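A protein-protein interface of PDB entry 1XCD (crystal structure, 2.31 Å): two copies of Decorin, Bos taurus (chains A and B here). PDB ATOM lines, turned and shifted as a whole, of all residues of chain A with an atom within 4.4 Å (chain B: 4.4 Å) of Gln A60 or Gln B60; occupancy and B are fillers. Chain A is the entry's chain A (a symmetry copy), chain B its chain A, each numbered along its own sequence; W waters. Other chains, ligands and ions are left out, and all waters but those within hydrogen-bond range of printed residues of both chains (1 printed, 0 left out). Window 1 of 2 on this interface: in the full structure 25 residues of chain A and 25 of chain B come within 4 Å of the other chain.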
ATOM      1  N   CYS A  38      -6.201   6.326   5.560  1.00  0.00           N
ATOM      2  CA  CYS A  38      -4.807   6.144   5.921  1.00  0.00           C
ATOM      3  C   CYS A  38      -4.602   5.961   7.423  1.00  0.00           C
ATOM      4  O   CYS A  38      -3.543   6.314   7.940  1.00  0.00           O
ATOM      5  CB  CYS A  38      -3.997   7.359   5.499  1.00  0.00           C
ATOM      6  SG  CYS A  38      -3.747   7.683   3.730  1.00  0.00           S
ATOM      7  N   SER A  39      -5.595   5.433   8.128  1.00  0.00           N
ATOM      8  CA  SER A  39      -5.447   5.215   9.566  1.00  0.00           C
ATOM      9  C   SER A  39      -4.428   4.133   9.855  1.00  0.00           C
ATOM     10  O   SER A  39      -4.097   3.328   8.992  1.00  0.00           O
ATOM     11  CB  SER A  39      -6.762   4.765  10.209  1.00  0.00           C
ATOM     12  OG  SER A  39      -7.787   5.719  10.056  1.00  0.00           O
ATOM     13  N   ASP A  40      -3.949   4.146  11.095  1.00  0.00           N
ATOM     14  CA  ASP A  40      -3.026   3.152  11.639  1.00  0.00           C
ATOM     15  C   ASP A  40      -1.769   2.843  10.840  1.00  0.00           C
ATOM     16  O   ASP A  40      -1.279   1.712  10.867  1.00  0.00           O
ATOM     17  CB  ASP A  40      -3.812   1.853  11.874  1.00  0.00           C
ATOM     18  CG  ASP A  40      -5.248   2.115  12.332  1.00  0.00           C
ATOM     19  OD1 ASP A  40      -6.186   1.614  11.677  1.00  0.00           O
ATOM     20  OD2 ASP A  40      -5.438   2.828  13.336  1.00  0.00           O
ATOM     21  N   ASP A  58      -9.041  10.363   6.171  1.00  0.00           N
ATOM     22  CA  ASP A  58      -8.877   9.777   7.505  1.00  0.00           C
ATOM     23  C   ASP A  58      -7.411   9.524   7.786  1.00  0.00           C
ATOM     24  O   ASP A  58      -6.809   8.617   7.199  1.00  0.00           O
ATOM     25  CB  ASP A  58      -9.645   8.449   7.592  1.00  0.00           C
ATOM     26  CG  ASP A  58      -9.867   7.981   9.034  1.00  0.00           C
ATOM     27  OD1 ASP A  58      -9.021   8.262   9.918  1.00  0.00           O
ATOM     28  OD2 ASP A  58     -10.892   7.311   9.283  1.00  0.00           O
ATOM     29  N   LEU A  59      -6.846  10.318   8.693  1.00  0.00           N
ATOM     30  CA  LEU A  59      -5.436  10.205   9.057  1.00  0.00           C
ATOM     31  C   LEU A  59      -5.276   9.842  10.538  1.00  0.00           C
ATOM     32  O   LEU A  59      -4.233  10.051  11.145  1.00  0.00           O
ATOM     33  CB  LEU A  59      -4.720  11.531   8.737  1.00  0.00           C
ATOM     34  CG  LEU A  59      -4.444  11.774   7.241  1.00  0.00           C
ATOM     35  CD1 LEU A  59      -4.105  13.239   6.948  1.00  0.00           C
ATOM     36  CD2 LEU A  59      -3.303  10.873   6.820  1.00  0.00           C
ATOM     37  N   GLN A  60      -6.324   9.270  11.101  1.00  0.00           N
ATOM     38  CA  GLN A  60      -6.350   8.871  12.498  1.00  0.00           C
ATOM     39  C   GLN A  60      -5.254   7.880  12.868  1.00  0.00           C
ATOM     40  O   GLN A  60      -4.837   7.075  12.052  1.00  0.00           O
ATOM     41  CB  GLN A  60      -7.706   8.246  12.782  1.00  0.00           C
ATOM     42  CG  GLN A  60      -7.994   7.985  14.221  1.00  0.00           C
ATOM     43  CD  GLN A  60      -9.466   7.747  14.449  1.00  0.00           C
ATOM     44  OE1 GLN A  60      -9.898   7.560  15.578  1.00  0.00           O
ATOM     45  NE2 GLN A  60     -10.248   7.758  13.373  1.00  0.00           N
ATOM     46  N   ASN A  61      -4.799   7.951  14.114  1.00  0.00           N
ATOM     47  CA  ASN A  61      -3.777   7.050  14.639  1.00  0.00           C
ATOM     48  C   ASN A  61      -2.501   6.953  13.818  1.00  0.00           C
ATOM     49  O   ASN A  61      -2.112   5.883  13.359  1.00  0.00           O
ATOM     50  CB  ASN A  61      -4.368   5.646  14.852  1.00  0.00           C
ATOM     51  CG  ASN A  61      -3.399   4.707  15.555  1.00  0.00           C
ATOM     52  OD1 ASN A  61      -2.599   5.144  16.379  1.00  0.00           O
ATOM     53  ND2 ASN A  61      -3.474   3.415  15.245  1.00  0.00           N
ATOM     54  N   ASN A  62      -1.852   8.088  13.622  1.00  0.00           N
ATOM     55  CA  ASN A  62      -0.589   8.124  12.898  1.00  0.00           C
ATOM     56  C   ASN A  62       0.389   8.873  13.794  1.00  0.00           C
ATOM     57  O   ASN A  62       0.109   9.052  14.983  1.00  0.00           O
ATOM     58  CB  ASN A  62      -0.767   8.814  11.548  1.00  0.00           C
ATOM     59  CG  ASN A  62      -1.255   7.865  10.484  1.00  0.00           C
ATOM     60  OD1 ASN A  62      -0.594   6.877  10.191  1.00  0.00           O
ATOM     61  ND2 ASN A  62      -2.417   8.152   9.899  1.00  0.00           N
ATOM     62  N   ILE A  82     -10.034  13.929   9.436  1.00  0.00           N
ATOM     63  CA  ILE A  82      -9.849  13.265  10.706  1.00  0.00           C
ATOM     64  C   ILE A  82      -8.367  13.142  10.982  1.00  0.00           C
ATOM     65  O   ILE A  82      -7.655  12.467  10.246  1.00  0.00           O
ATOM     66  CB  ILE A  82     -10.509  11.861  10.673  1.00  0.00           C
ATOM     67  CG1 ILE A  82     -11.983  12.004  10.281  1.00  0.00           C
ATOM     68  CG2 ILE A  82     -10.382  11.187  12.038  1.00  0.00           C
ATOM     69  CD1 ILE A  82     -12.697  10.693  10.066  1.00  0.00           C
ATOM     70  N   ILE A  84      -7.509  12.759  14.360  1.00  0.00           N
ATOM     71  CA  ILE A  84      -7.581  12.206  15.698  1.00  0.00           C
ATOM     72  C   ILE A  84      -6.392  11.286  15.971  1.00  0.00           C
ATOM     73  O   ILE A  84      -5.950  10.542  15.095  1.00  0.00           O
ATOM     74  CB  ILE A  84      -8.871  11.371  15.876  1.00  0.00           C
ATOM     75  CG1 ILE A  84     -10.109  12.264  15.853  1.00  0.00           C
ATOM     76  CG2 ILE A  84      -8.815  10.579  17.192  1.00  0.00           C
ATOM     77  CD1 ILE A  84     -11.428  11.448  15.799  1.00  0.00           C
ATOM     78  N   CYS B  38     -21.563  10.545  19.847  1.00  0.00           N
ATOM     79  CA  CYS B  38     -21.388  10.373  21.278  1.00  0.00           C
ATOM     80  C   CYS B  38     -19.928  10.181  21.678  1.00  0.00           C
ATOM     81  O   CYS B  38     -19.654   9.527  22.684  1.00  0.00           O
ATOM     82  CB  CYS B  38     -22.153   9.148  21.752  1.00  0.00           C
ATOM     83  SG  CYS B  38     -23.968   9.177  21.733  1.00  0.00           S
ATOM     84  N   SER B  39     -18.993  10.722  20.906  1.00  0.00           N
ATOM     85  CA  SER B  39     -17.579  10.588  21.252  1.00  0.00           C
ATOM     86  C   SER B  39     -17.245  11.364  22.508  1.00  0.00           C
ATOM     87  O   SER B  39     -17.977  12.260  22.912  1.00  0.00           O
ATOM     88  CB  SER B  39     -16.671  11.130  20.144  1.00  0.00           C
ATOM     89  OG  SER B  39     -16.848  10.446  18.925  1.00  0.00           O
ATOM     90  N   ASP B  40     -16.117  10.988  23.103  1.00  0.00           N
ATOM     91  CA  ASP B  40     -15.538  11.643  24.274  1.00  0.00           C
ATOM     92  C   ASP B  40     -16.444  11.873  25.475  1.00  0.00           C
ATOM     93  O   ASP B  40     -16.274  12.855  26.200  1.00  0.00           O
ATOM     94  CB  ASP B  40     -14.942  12.986  23.821  1.00  0.00           C
ATOM     95  CG  ASP B  40     -14.333  12.910  22.420  1.00  0.00           C
ATOM     96  OD1 ASP B  40     -14.731  13.713  21.550  1.00  0.00           O
ATOM     97  OD2 ASP B  40     -13.467  12.044  22.188  1.00  0.00           O
ATOM     98  N   ASP B  58     -21.316   7.093  16.276  1.00  0.00           N
ATOM     99  CA  ASP B  58     -19.936   7.330  16.706  1.00  0.00           C
ATOM    100  C   ASP B  58     -19.835   7.230  18.213  1.00  0.00           C
ATOM    101  O   ASP B  58     -20.321   8.111  18.933  1.00  0.00           O
ATOM    102  CB  ASP B  58     -19.480   8.729  16.261  1.00  0.00           C
ATOM    103  CG  ASP B  58     -17.959   8.904  16.303  1.00  0.00           C
ATOM    104  OD1 ASP B  58     -17.283   8.280  17.156  1.00  0.00           O
ATOM    105  OD2 ASP B  58     -17.434   9.687  15.482  1.00  0.00           O
ATOM    106  N   LEU B  59     -19.193   6.164  18.685  1.00  0.00           N
ATOM    107  CA  LEU B  59     -19.031   5.923  20.116  1.00  0.00           C
ATOM    108  C   LEU B  59     -17.549   5.915  20.510  1.00  0.00           C
ATOM    109  O   LEU B  59     -17.157   5.382  21.541  1.00  0.00           O
ATOM    110  CB  LEU B  59     -19.703   4.586  20.486  1.00  0.00           C
ATOM    111  CG  LEU B  59     -21.242   4.629  20.540  1.00  0.00           C
ATOM    112  CD1 LEU B  59     -21.858   3.226  20.516  1.00  0.00           C
ATOM    113  CD2 LEU B  59     -21.649   5.364  21.798  1.00  0.00           C
ATOM    114  N   GLN B  60     -16.735   6.540  19.679  1.00  0.00           N
ATOM    115  CA  GLN B  60     -15.300   6.621  19.891  1.00  0.00           C
ATOM    116  C   GLN B  60     -14.916   7.278  21.211  1.00  0.00           C
ATOM    117  O   GLN B  60     -15.616   8.146  21.704  1.00  0.00           O
ATOM    118  CB  GLN B  60     -14.700   7.417  18.743  1.00  0.00           C
ATOM    119  CG  GLN B  60     -13.211   7.406  18.676  1.00  0.00           C
ATOM    120  CD  GLN B  60     -12.723   7.866  17.325  1.00  0.00           C
ATOM    121  OE1 GLN B  60     -11.527   7.881  17.068  1.00  0.00           O
ATOM    122  NE2 GLN B  60     -13.651   8.242  16.448  1.00  0.00           N
ATOM    123  N   ASN B  61     -13.790   6.851  21.770  1.00  0.00           N
ATOM    124  CA  ASN B  61     -13.263   7.401  23.015  1.00  0.00           C
ATOM    125  C   ASN B  61     -14.233   7.430  24.186  1.00  0.00           C
ATOM    126  O   ASN B  61     -14.531   8.479  24.747  1.00  0.00           O
ATOM    127  CB  ASN B  61     -12.697   8.812  22.772  1.00  0.00           C
ATOM    128  CG  ASN B  61     -11.982   9.370  23.992  1.00  0.00           C
ATOM    129  OD1 ASN B  61     -11.387   8.619  24.762  1.00  0.00           O
ATOM    130  ND2 ASN B  61     -12.024  10.689  24.170  1.00  0.00           N
ATOM    131  N   ASN B  62     -14.738   6.262  24.546  1.00  0.00           N
ATOM    132  CA  ASN B  62     -15.637   6.144  25.685  1.00  0.00           C
ATOM    133  C   ASN B  62     -15.059   5.044  26.565  1.00  0.00           C
ATOM    134  O   ASN B  62     -13.898   4.666  26.383  1.00  0.00           O
ATOM    135  CB  ASN B  62     -17.052   5.813  25.216  1.00  0.00           C
ATOM    136  CG  ASN B  62     -17.828   7.048  24.837  1.00  0.00           C
ATOM    137  OD1 ASN B  62     -18.023   7.930  25.662  1.00  0.00           O
ATOM    138  ND2 ASN B  62     -18.275   7.123  23.583  1.00  0.00           N
ATOM    139  N   ILE B  82     -18.684   3.157  14.883  1.00  0.00           N
ATOM    140  CA  ILE B  82     -17.353   3.480  15.344  1.00  0.00           C
ATOM    141  C   ILE B  82     -17.285   3.253  16.838  1.00  0.00           C
ATOM    142  O   ILE B  82     -17.976   3.923  17.597  1.00  0.00           O
ATOM    143  CB  ILE B  82     -17.016   4.956  15.008  1.00  0.00           C
ATOM    144  CG1 ILE B  82     -17.202   5.188  13.504  1.00  0.00           C
ATOM    145  CG2 ILE B  82     -15.582   5.278  15.424  1.00  0.00           C
ATOM    146  CD1 ILE B  82     -17.051   6.625  13.076  1.00  0.00           C
ATOM    147  N   ILE B  84     -14.064   2.716  18.116  1.00  0.00           N
ATOM    148  CA  ILE B  84     -12.650   2.965  18.311  1.00  0.00           C
ATOM    149  C   ILE B  84     -12.389   3.558  19.695  1.00  0.00           C
ATOM    150  O   ILE B  84     -13.162   4.378  20.193  1.00  0.00           O
ATOM    151  CB  ILE B  84     -12.123   3.973  17.262  1.00  0.00           C
ATOM    152  CG1 ILE B  84     -12.130   3.360  15.864  1.00  0.00           C
ATOM    153  CG2 ILE B  84     -10.703   4.431  17.631  1.00  0.00           C
ATOM    154  CD1 ILE B  84     -11.827   4.405  14.758  1.00  0.00           C
HETATM  155  O   HOH W   1     -13.029   8.246  13.675  1.00  0.00           O
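The backbone NH of Asn B61 lies within hydrogen-bond range of the backbone carbonyl oxygen of Ile B84 (3.0 Å). The backbone NH (N) of Asn A61 is in hydrogen-bond range of the backbone carbonyl oxygen (O) of Ile A84 (3.0 Å). N of Asp B40 lies within hydrogen-bond range of O of Gln B60 (3.2 Å). The side-chain amide nitrogen (ND2) of Asn A62 sits at hydrogen-bond distance from the backbone carbonyl oxygen (O) of Gln A60, 3.4 Å away. The backbone NH (N) of Gln A60 lies within hydrogen-bond range of the side-chain carboxylate (OD1) of Asp A58 (3.1 Å). The side-chain amide nitrogen of Asn B62 sits at hydrogen-bond distance from the backbone carbonyl oxygen of Gln B60, at 3.4 Å.
Water W1 bridges NE2 of Gln A60 and NE2 of Gln B60.
Of chain B, only Gln B60 (2.2 Å) and Ile B84 (3.8 Å) come within 4 Å of Gln A60. Of the printed residues of chain B, Ile A84 touches Gln B60. Gln B60 touches just these residues of chain A: Gln A60 and Ile A84. Printed residues of chain A within 4 Å of Ile B84: Gln A60. The nearest printed residue of chain B that does not touch Gln A60 is Ile B82 (6.1 Å). The nearest printed residue of chain A that does not touch Gln B60 is Ile A82 (6.1 Å). The nearest printed residue of chain A that does not touch Ile B84 is Asp A58 (6.3 Å).
Gln A60 touches its own counterpart, Gln B60. Gln A60 touches Ile B84, and with the chains exchanged Ile A84 touches Gln B60. 10 positions are printed for both chains. Of the 3 pairs that touch across the chains among the printed residues, 3 have their exchanged pair printed and touching as well.
Hydrophobic or aromatic side chains of chain A that line the printed part of chain B: Ile A84. Of the 10 printed residues of chain B, 2 touch a printed residue of chain A. Among the printed residues, 3 pairs touch across the chains.
Gln A60 touches Ile B84 (OE1 to CD1, 3.8 Å). Ile A84 touches Gln B60.
The side-chain amide oxygen (OE1) of Gln A60 lies close to the side-chain amide oxygen (OE1) of Gln B60, 2.2 Å away.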
